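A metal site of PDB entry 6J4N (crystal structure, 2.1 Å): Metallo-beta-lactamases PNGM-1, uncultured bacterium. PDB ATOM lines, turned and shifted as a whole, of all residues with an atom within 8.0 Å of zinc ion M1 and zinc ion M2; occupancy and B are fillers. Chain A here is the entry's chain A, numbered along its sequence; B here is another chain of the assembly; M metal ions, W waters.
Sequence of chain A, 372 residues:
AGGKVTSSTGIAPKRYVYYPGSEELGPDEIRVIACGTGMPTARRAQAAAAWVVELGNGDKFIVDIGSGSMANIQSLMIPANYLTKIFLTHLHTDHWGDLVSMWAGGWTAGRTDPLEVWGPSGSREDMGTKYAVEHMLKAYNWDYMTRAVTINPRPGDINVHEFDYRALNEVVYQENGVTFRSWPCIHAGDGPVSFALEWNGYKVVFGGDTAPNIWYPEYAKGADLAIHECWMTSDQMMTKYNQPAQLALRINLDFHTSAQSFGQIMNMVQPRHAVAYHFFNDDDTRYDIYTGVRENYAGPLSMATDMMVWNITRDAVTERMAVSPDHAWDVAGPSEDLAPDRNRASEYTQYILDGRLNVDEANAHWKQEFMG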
ATOM      1  N   GLY A  38     -12.297 -13.544  25.224  1.00  0.00           N
ATOM      2  CA  GLY A  38     -13.506 -13.228  24.457  1.00  0.00           C
ATOM      3  C   GLY A  38     -14.699 -14.111  24.757  1.00  0.00           C
ATOM      4  O   GLY A  38     -14.935 -14.422  25.911  1.00  0.00           O
ATOM      5  N   MET A  39     -15.474 -14.464  23.730  1.00  0.00           N
ATOM      6  CA  MET A  39     -16.880 -14.943  23.850  1.00  0.00           C
ATOM      7  C   MET A  39     -17.047 -16.148  22.943  1.00  0.00           C
ATOM      8  O   MET A  39     -16.144 -16.426  22.161  1.00  0.00           O
ATOM      9  CB  MET A  39     -17.825 -13.859  23.325  1.00  0.00           C
ATOM     10  CG  MET A  39     -17.805 -12.586  24.089  1.00  0.00           C
ATOM     11  SD  MET A  39     -18.900 -12.811  25.501  1.00  0.00           S
ATOM     12  CE  MET A  39     -19.812 -11.288  25.294  1.00  0.00           C
ATOM     13  N   PRO A  40     -18.244 -16.792  22.848  1.00  0.00           N
ATOM     14  CA  PRO A  40     -18.432 -17.840  21.846  1.00  0.00           C
ATOM     15  C   PRO A  40     -18.603 -17.262  20.437  1.00  0.00           C
ATOM     16  O   PRO A  40     -18.526 -18.004  19.478  1.00  0.00           O
ATOM     17  CB  PRO A  40     -19.711 -18.576  22.255  1.00  0.00           C
ATOM     18  CG  PRO A  40     -20.435 -17.612  23.172  1.00  0.00           C
ATOM     19  CD  PRO A  40     -19.482 -16.493  23.579  1.00  0.00           C
ATOM     20  N   ALA A  48     -11.379 -16.995  22.281  1.00  0.00           N
ATOM     21  CA  ALA A  48     -12.171 -17.456  23.442  1.00  0.00           C
ATOM     22  C   ALA A  48     -11.213 -17.766  24.592  1.00  0.00           C
ATOM     23  O   ALA A  48     -10.015 -18.020  24.365  1.00  0.00           O
ATOM     24  CB  ALA A  48     -12.990 -18.644  23.096  1.00  0.00           C
ATOM     25  N   ALA A  49     -11.764 -17.787  25.791  1.00  0.00           N
ATOM     26  CA  ALA A  49     -11.077 -17.997  27.075  1.00  0.00           C
ATOM     27  C   ALA A  49      -9.933 -19.001  27.048  1.00  0.00           C
ATOM     28  O   ALA A  49     -10.181 -20.198  26.737  1.00  0.00           O
ATOM     29  CB  ALA A  49     -12.104 -18.491  28.036  1.00  0.00           C
ATOM     30  N   ASP A  64      -8.276 -23.473  30.669  1.00  0.00           N
ATOM     31  CA  ASP A  64      -9.190 -23.165  29.543  1.00  0.00           C
ATOM     32  C   ASP A  64      -8.391 -23.031  28.231  1.00  0.00           C
ATOM     33  O   ASP A  64      -7.234 -22.579  28.234  1.00  0.00           O
ATOM     34  CB  ASP A  64     -10.108 -21.959  29.827  1.00  0.00           C
ATOM     35  CG  ASP A  64     -11.220 -22.300  30.790  1.00  0.00           C
ATOM     36  OD1 ASP A  64     -11.384 -23.495  31.046  1.00  0.00           O
ATOM     37  OD2 ASP A  64     -11.929 -21.362  31.295  1.00  0.00           O
ATOM     38  N   THR A  89     -12.461 -25.147  33.092  1.00  0.00           N
ATOM     39  CA  THR A  89     -13.466 -24.656  34.063  1.00  0.00           C
ATOM     40  C   THR A  89     -14.852 -25.217  33.756  1.00  0.00           C
ATOM     41  O   THR A  89     -15.607 -25.469  34.676  1.00  0.00           O
ATOM     42  CB  THR A  89     -13.549 -23.136  34.069  1.00  0.00           C
ATOM     43  OG1 THR A  89     -13.953 -22.725  32.762  1.00  0.00           O
ATOM     44  CG2 THR A  89     -12.251 -22.527  34.544  1.00  0.00           C
ATOM     45  N   HIS A  90     -15.196 -25.328  32.499  1.00  0.00           N
ATOM     46  CA  HIS A  90     -16.482 -25.937  32.106  1.00  0.00           C
ATOM     47  C   HIS A  90     -16.442 -26.275  30.619  1.00  0.00           C
ATOM     48  O   HIS A  90     -15.460 -25.992  29.935  1.00  0.00           O
ATOM     49  CB  HIS A  90     -17.659 -25.001  32.404  1.00  0.00           C
ATOM     50  CG  HIS A  90     -17.621 -23.696  31.694  1.00  0.00           C
ATOM     51  ND1 HIS A  90     -16.607 -22.792  31.881  1.00  0.00           N
ATOM     52  CD2 HIS A  90     -18.523 -23.078  30.893  1.00  0.00           C
ATOM     53  CE1 HIS A  90     -16.887 -21.690  31.216  1.00  0.00           C
ATOM     54  NE2 HIS A  90     -18.036 -21.832  30.613  1.00  0.00           N
ATOM     55  N   LEU A  91     -17.520 -26.849  30.117  1.00  0.00           N
ATOM     56  CA  LEU A  91     -17.504 -27.554  28.810  1.00  0.00           C
ATOM     57  C   LEU A  91     -18.207 -26.802  27.691  1.00  0.00           C
ATOM     58  O   LEU A  91     -18.551 -27.402  26.663  1.00  0.00           O
ATOM     59  CB  LEU A  91     -18.095 -28.942  29.036  1.00  0.00           C
ATOM     60  CG  LEU A  91     -17.290 -29.847  29.970  1.00  0.00           C
ATOM     61  CD1 LEU A  91     -18.104 -31.099  30.268  1.00  0.00           C
ATOM     62  CD2 LEU A  91     -15.927 -30.258  29.398  1.00  0.00           C
ATOM     63  N   HIS A  92     -18.380 -25.506  27.843  1.00  0.00           N
ATOM     64  CA  HIS A  92     -18.744 -24.619  26.720  1.00  0.00           C
ATOM     65  C   HIS A  92     -17.629 -24.580  25.678  1.00  0.00           C
ATOM     66  O   HIS A  92     -16.476 -24.586  26.069  1.00  0.00           O
ATOM     67  CB  HIS A  92     -19.027 -23.220  27.214  1.00  0.00           C
ATOM     68  CG  HIS A  92     -20.431 -23.007  27.632  1.00  0.00           C
ATOM     69  ND1 HIS A  92     -20.771 -22.109  28.631  1.00  0.00           N
ATOM     70  CD2 HIS A  92     -21.595 -23.486  27.130  1.00  0.00           C
ATOM     71  CE1 HIS A  92     -22.100 -22.113  28.761  1.00  0.00           C
ATOM     72  NE2 HIS A  92     -22.609 -22.942  27.870  1.00  0.00           N
ATOM     73  N   THR A  93     -17.973 -24.580  24.390  1.00  0.00           N
ATOM     74  CA  THR A  93     -17.006 -24.439  23.274  1.00  0.00           C
ATOM     75  C   THR A  93     -16.028 -23.295  23.509  1.00  0.00           C
ATOM     76  O   THR A  93     -14.881 -23.445  23.154  1.00  0.00           O
ATOM     77  CB  THR A  93     -17.679 -24.160  21.927  1.00  0.00           C
ATOM     78  OG1 THR A  93     -18.167 -22.816  21.930  1.00  0.00           O
ATOM     79  CG2 THR A  93     -18.824 -25.120  21.684  1.00  0.00           C
ATOM     80  N   ASP A  94     -16.432 -22.169  24.076  1.00  0.00           N
ATOM     81  CA  ASP A  94     -15.435 -21.068  24.207  1.00  0.00           C
ATOM     82  C   ASP A  94     -14.452 -21.339  25.358  1.00  0.00           C
ATOM     83  O   ASP A  94     -13.616 -20.452  25.684  1.00  0.00           O
ATOM     84  CB  ASP A  94     -16.146 -19.709  24.268  1.00  0.00           C
ATOM     85  CG  ASP A  94     -17.174 -19.582  25.353  1.00  0.00           C
ATOM     86  OD1 ASP A  94     -17.103 -18.581  26.082  1.00  0.00           O
ATOM     87  OD2 ASP A  94     -18.027 -20.499  25.460  1.00  0.00           O
ATOM     88  N   HIS A  95     -14.489 -22.530  25.970  1.00  0.00           N
ATOM     89  CA  HIS A  95     -13.551 -22.867  27.050  1.00  0.00           C
ATOM     90  C   HIS A  95     -12.733 -24.125  26.736  1.00  0.00           C
ATOM     91  O   HIS A  95     -11.705 -24.319  27.425  1.00  0.00           O
ATOM     92  CB  HIS A  95     -14.326 -22.890  28.368  1.00  0.00           C
ATOM     93  CG  HIS A  95     -14.683 -21.505  28.809  1.00  0.00           C
ATOM     94  ND1 HIS A  95     -13.967 -20.822  29.767  1.00  0.00           N
ATOM     95  CD2 HIS A  95     -15.673 -20.685  28.426  1.00  0.00           C
ATOM     96  CE1 HIS A  95     -14.489 -19.612  29.926  1.00  0.00           C
ATOM     97  NE2 HIS A  95     -15.527 -19.519  29.116  1.00  0.00           N
ATOM     98  N   HIS A 187     -23.852 -21.365  36.313  1.00  0.00           N
ATOM     99  CA  HIS A 187     -23.611 -21.055  34.893  1.00  0.00           C
ATOM    100  C   HIS A 187     -24.219 -22.134  33.994  1.00  0.00           C
ATOM    101  O   HIS A 187     -23.604 -23.232  33.863  1.00  0.00           O
ATOM    102  CB  HIS A 187     -22.090 -20.912  34.696  1.00  0.00           C
ATOM    103  CG  HIS A 187     -21.734 -20.569  33.299  1.00  0.00           C
ATOM    104  ND1 HIS A 187     -22.002 -19.335  32.751  1.00  0.00           N
ATOM    105  CD2 HIS A 187     -21.154 -21.306  32.334  1.00  0.00           C
ATOM    106  CE1 HIS A 187     -21.610 -19.331  31.509  1.00  0.00           C
ATOM    107  NE2 HIS A 187     -21.072 -20.531  31.236  1.00  0.00           N
ATOM    108  N   ALA A 188     -25.399 -21.824  33.451  1.00  0.00           N
ATOM    109  CA  ALA A 188     -26.222 -22.573  32.455  1.00  0.00           C
ATOM    110  C   ALA A 188     -26.788 -23.907  32.981  1.00  0.00           C
ATOM    111  O   ALA A 188     -27.877 -24.291  32.560  1.00  0.00           O
ATOM    112  CB  ALA A 188     -25.474 -22.794  31.161  1.00  0.00           C
ATOM    113  N   PRO A 192     -19.990 -26.388  35.949  1.00  0.00           N
ATOM    114  CA  PRO A 192     -18.919 -25.412  35.888  1.00  0.00           C
ATOM    115  C   PRO A 192     -18.302 -25.118  37.246  1.00  0.00           C
ATOM    116  O   PRO A 192     -18.990 -25.104  38.238  1.00  0.00           O
ATOM    117  CB  PRO A 192     -19.618 -24.160  35.343  1.00  0.00           C
ATOM    118  CG  PRO A 192     -20.695 -24.721  34.435  1.00  0.00           C
ATOM    119  CD  PRO A 192     -21.162 -25.953  35.191  1.00  0.00           C
ATOM    120  N   GLY A 208     -13.365 -18.817  35.649  1.00  0.00           N
ATOM    121  CA  GLY A 208     -14.230 -19.421  34.618  1.00  0.00           C
ATOM    122  C   GLY A 208     -15.450 -18.556  34.373  1.00  0.00           C
ATOM    123  O   GLY A 208     -15.303 -17.303  34.304  1.00  0.00           O
ATOM    124  N   ASP A 209     -16.628 -19.166  34.267  1.00  0.00           N
ATOM    125  CA  ASP A 209     -17.882 -18.415  34.051  1.00  0.00           C
ATOM    126  C   ASP A 209     -18.851 -18.640  35.206  1.00  0.00           C
ATOM    127  O   ASP A 209     -19.017 -19.795  35.616  1.00  0.00           O
ATOM    128  CB  ASP A 209     -18.616 -18.856  32.792  1.00  0.00           C
ATOM    129  CG  ASP A 209     -17.947 -18.481  31.470  1.00  0.00           C
ATOM    130  OD1 ASP A 209     -16.878 -17.835  31.486  1.00  0.00           O
ATOM    131  OD2 ASP A 209     -18.512 -18.870  30.429  1.00  0.00           O
ATOM    132  N   THR A 210     -19.542 -17.576  35.603  1.00  0.00           N
ATOM    133  CA  THR A 210     -20.594 -17.677  36.626  1.00  0.00           C
ATOM    134  C   THR A 210     -21.399 -16.377  36.793  1.00  0.00           C
ATOM    135  O   THR A 210     -20.836 -15.269  36.612  1.00  0.00           O
ATOM    136  CB  THR A 210     -19.946 -18.112  37.942  1.00  0.00           C
ATOM    137  OG1 THR A 210     -20.921 -18.439  38.927  1.00  0.00           O
ATOM    138  CG2 THR A 210     -19.045 -17.015  38.464  1.00  0.00           C
ATOM    139  N   GLU A 229     -15.370 -13.414  35.591  1.00  0.00           N
ATOM    140  CA  GLU A 229     -16.273 -12.980  34.519  1.00  0.00           C
ATOM    141  C   GLU A 229     -16.759 -11.567  34.864  1.00  0.00           C
ATOM    142  O   GLU A 229     -17.019 -11.289  36.035  1.00  0.00           O
ATOM    143  CB  GLU A 229     -17.403 -14.002  34.348  1.00  0.00           C
ATOM    144  CG  GLU A 229     -18.679 -13.391  33.799  1.00  0.00           C
ATOM    145  CD  GLU A 229     -19.862 -14.302  33.609  1.00  0.00           C
ATOM    146  OE1 GLU A 229     -19.683 -15.558  33.472  1.00  0.00           O
ATOM    147  OE2 GLU A 229     -20.961 -13.751  33.532  1.00  0.00           O
ATOM    148  N   TRP A 231     -19.397  -8.786  32.785  1.00  0.00           N
ATOM    149  CA  TRP A 231     -20.248  -8.802  31.572  1.00  0.00           C
ATOM    150  C   TRP A 231     -20.384  -7.408  30.964  1.00  0.00           C
ATOM    151  O   TRP A 231     -20.340  -6.406  31.679  1.00  0.00           O
ATOM    152  CB  TRP A 231     -21.621  -9.397  31.832  1.00  0.00           C
ATOM    153  CG  TRP A 231     -22.153 -10.123  30.635  1.00  0.00           C
ATOM    154  CD1 TRP A 231     -23.266  -9.822  29.900  1.00  0.00           C
ATOM    155  CD2 TRP A 231     -21.599 -11.312  30.055  1.00  0.00           C
ATOM    156  NE1 TRP A 231     -23.451 -10.754  28.903  1.00  0.00           N
ATOM    157  CE2 TRP A 231     -22.439 -11.680  28.979  1.00  0.00           C
ATOM    158  CE3 TRP A 231     -20.504 -12.127  30.372  1.00  0.00           C
ATOM    159  CZ2 TRP A 231     -22.187 -12.797  28.189  1.00  0.00           C
ATOM    160  CZ3 TRP A 231     -20.253 -13.244  29.582  1.00  0.00           C
ATOM    161  CH2 TRP A 231     -21.079 -13.559  28.505  1.00  0.00           C
ATOM    162  N   HIS A 256     -25.462 -13.597  34.279  1.00  0.00           N
ATOM    163  CA  HIS A 256     -24.040 -13.158  34.231  1.00  0.00           C
ATOM    164  C   HIS A 256     -23.681 -12.301  35.426  1.00  0.00           C
ATOM    165  O   HIS A 256     -24.587 -11.808  36.150  1.00  0.00           O
ATOM    166  CB  HIS A 256     -23.750 -12.451  32.907  1.00  0.00           C
ATOM    167  CG  HIS A 256     -23.846 -13.374  31.745  1.00  0.00           C
ATOM    168  ND1 HIS A 256     -22.849 -14.302  31.468  1.00  0.00           N
ATOM    169  CD2 HIS A 256     -24.818 -13.569  30.827  1.00  0.00           C
ATOM    170  CE1 HIS A 256     -23.214 -15.018  30.425  1.00  0.00           C
ATOM    171  NE2 HIS A 256     -24.412 -14.570  29.992  1.00  0.00           N
ATOM    172  N   TYR A 277     -12.635 -10.186  32.825  1.00  0.00           N
ATOM    173  CA  TYR A 277     -12.518 -10.723  31.451  1.00  0.00           C
ATOM    174  C   TYR A 277     -13.893 -11.153  30.966  1.00  0.00           C
ATOM    175  O   TYR A 277     -14.883 -11.067  31.723  1.00  0.00           O
ATOM    176  CB  TYR A 277     -11.479 -11.870  31.371  1.00  0.00           C
ATOM    177  CG  TYR A 277     -12.041 -13.260  31.587  1.00  0.00           C
ATOM    178  CD1 TYR A 277     -12.555 -13.637  32.810  1.00  0.00           C
ATOM    179  CD2 TYR A 277     -12.076 -14.193  30.564  1.00  0.00           C
ATOM    180  CE1 TYR A 277     -13.071 -14.910  33.014  1.00  0.00           C
ATOM    181  CE2 TYR A 277     -12.633 -15.454  30.741  1.00  0.00           C
ATOM    182  CZ  TYR A 277     -13.115 -15.816  31.969  1.00  0.00           C
ATOM    183  OH  TYR A 277     -13.653 -17.055  32.155  1.00  0.00           O
ATOM    184  N   HIS A 278     -13.888 -11.591  29.704  1.00  0.00           N
ATOM    185  CA  HIS A 278     -15.005 -12.267  28.989  1.00  0.00           C
ATOM    186  C   HIS A 278     -16.071 -11.254  28.576  1.00  0.00           C
ATOM    187  O   HIS A 278     -17.247 -11.561  28.601  1.00  0.00           O
ATOM    188  CB  HIS A 278     -15.590 -13.359  29.893  1.00  0.00           C
ATOM    189  CG  HIS A 278     -16.266 -14.465  29.182  1.00  0.00           C
ATOM    190  ND1 HIS A 278     -17.301 -14.271  28.271  1.00  0.00           N
ATOM    191  CD2 HIS A 278     -16.135 -15.797  29.338  1.00  0.00           C
ATOM    192  CE1 HIS A 278     -17.734 -15.458  27.861  1.00  0.00           C
ATOM    193  NE2 HIS A 278     -17.046 -16.411  28.521  1.00  0.00           N
ATOM    194  N   TRP B 142     -22.913 -31.443  27.171  1.00  0.00           N
ATOM    195  CA  TRP B 142     -23.172 -30.472  28.279  1.00  0.00           C
ATOM    196  C   TRP B 142     -23.645 -29.123  27.722  1.00  0.00           C
ATOM    197  O   TRP B 142     -24.666 -28.574  28.199  1.00  0.00           O
ATOM    198  CB  TRP B 142     -21.956 -30.288  29.185  1.00  0.00           C
ATOM    199  CG  TRP B 142     -22.259 -29.380  30.349  1.00  0.00           C
ATOM    200  CD1 TRP B 142     -22.722 -29.757  31.583  1.00  0.00           C
ATOM    201  CD2 TRP B 142     -22.146 -27.953  30.383  1.00  0.00           C
ATOM    202  NE1 TRP B 142     -22.926 -28.644  32.348  1.00  0.00           N
ATOM    203  CE2 TRP B 142     -22.570 -27.528  31.662  1.00  0.00           C
ATOM    204  CE3 TRP B 142     -21.703 -26.990  29.477  1.00  0.00           C
ATOM    205  CZ2 TRP B 142     -22.603 -26.188  32.023  1.00  0.00           C
ATOM    206  CZ3 TRP B 142     -21.726 -25.664  29.840  1.00  0.00           C
ATOM    207  CH2 TRP B 142     -22.143 -25.271  31.103  1.00  0.00           C
ATOM    208  N   ASP B 143     -22.928 -28.619  26.727  1.00  0.00           N
ATOM    209  CA  ASP B 143     -23.219 -27.342  26.037  1.00  0.00           C
ATOM    210  C   ASP B 143     -24.629 -27.450  25.436  1.00  0.00           C
ATOM    211  O   ASP B 143     -25.479 -26.593  25.729  1.00  0.00           O
ATOM    212  CB  ASP B 143     -22.110 -27.088  24.986  1.00  0.00           C
ATOM    213  CG  ASP B 143     -22.133 -25.715  24.332  1.00  0.00           C
ATOM    214  OD1 ASP B 143     -23.177 -25.322  23.882  1.00  0.00           O
ATOM    215  OD2 ASP B 143     -21.061 -25.043  24.283  1.00  0.00           O
HETATM  216 ZN    ZN M   1     -17.622 -18.585  28.453  1.00  0.00          ZN
HETATM  217 ZN    ZN M   2     -19.680 -20.580  29.605  1.00  0.00          ZN
HETATM  218  O   HOH W   1     -20.482 -18.182  28.046  1.00  0.00           O
HETATM  219  O   HOH W   2     -18.719 -20.232  27.882  1.00  0.00           O
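A ring nitrogen (ND1) of His 278 sits at hydrogen-bond distance from the backbone carbonyl oxygen of Gly 38 (3.3 Å).
O of Asp 94 is in hydrogen-bond range of N of Ala 49 (3.2 Å).
The side-chain sulfur of Met 39 lies within hydrogen-bond range of a ring nitrogen (ND1) of His 278.
ND1 of His 90 lies within hydrogen-bond range of OG1 of Thr 89 (2.8 Å).
The side-chain carboxylate (OD2) of Asp 64 lies within hydrogen-bond range of a ring nitrogen (ND1) of His 95 (2.6 Å).
The side-chain hydroxyl (OH) of Tyr 277 lies within hydrogen-bond range of the side-chain carboxylate (OD1) of Asp 209 (3.4 Å).
Five residues have an atom within 4 Å of zinc ion M1: His 90, Asp 94, His 95, Asp 209 and His 278.
The nearest printed residue that does not touch zinc ion M1 is His 92 (4.7 Å).
Four residues have an atom within 4 Å of zinc ion M2: His 90, His 92, His 187 and Asp 209.
Zinc ion M1 is bound by water W2 (2.1 Å), OD2 of Asp 209 (2.2 Å), NE2 of His 278 (2.3 Å), NE2 of His 95 (2.4 Å) and OD1 of Asp 94 (2.4 Å).
Zinc ion M1 has five donor atoms within binding distance.
Water W2 binds zinc ion M2 (2.0 Å).
ND1 of His 92 binds zinc ion M2 (2.1 Å).
A ring nitrogen (NE2) of His 187 is bound to zinc ion M2 (2.1 Å).
Zinc ion M2 is bound by OD2 of Asp 209 (2.2 Å).
NE2 of His 90 binds zinc ion M2 (2.3 Å).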
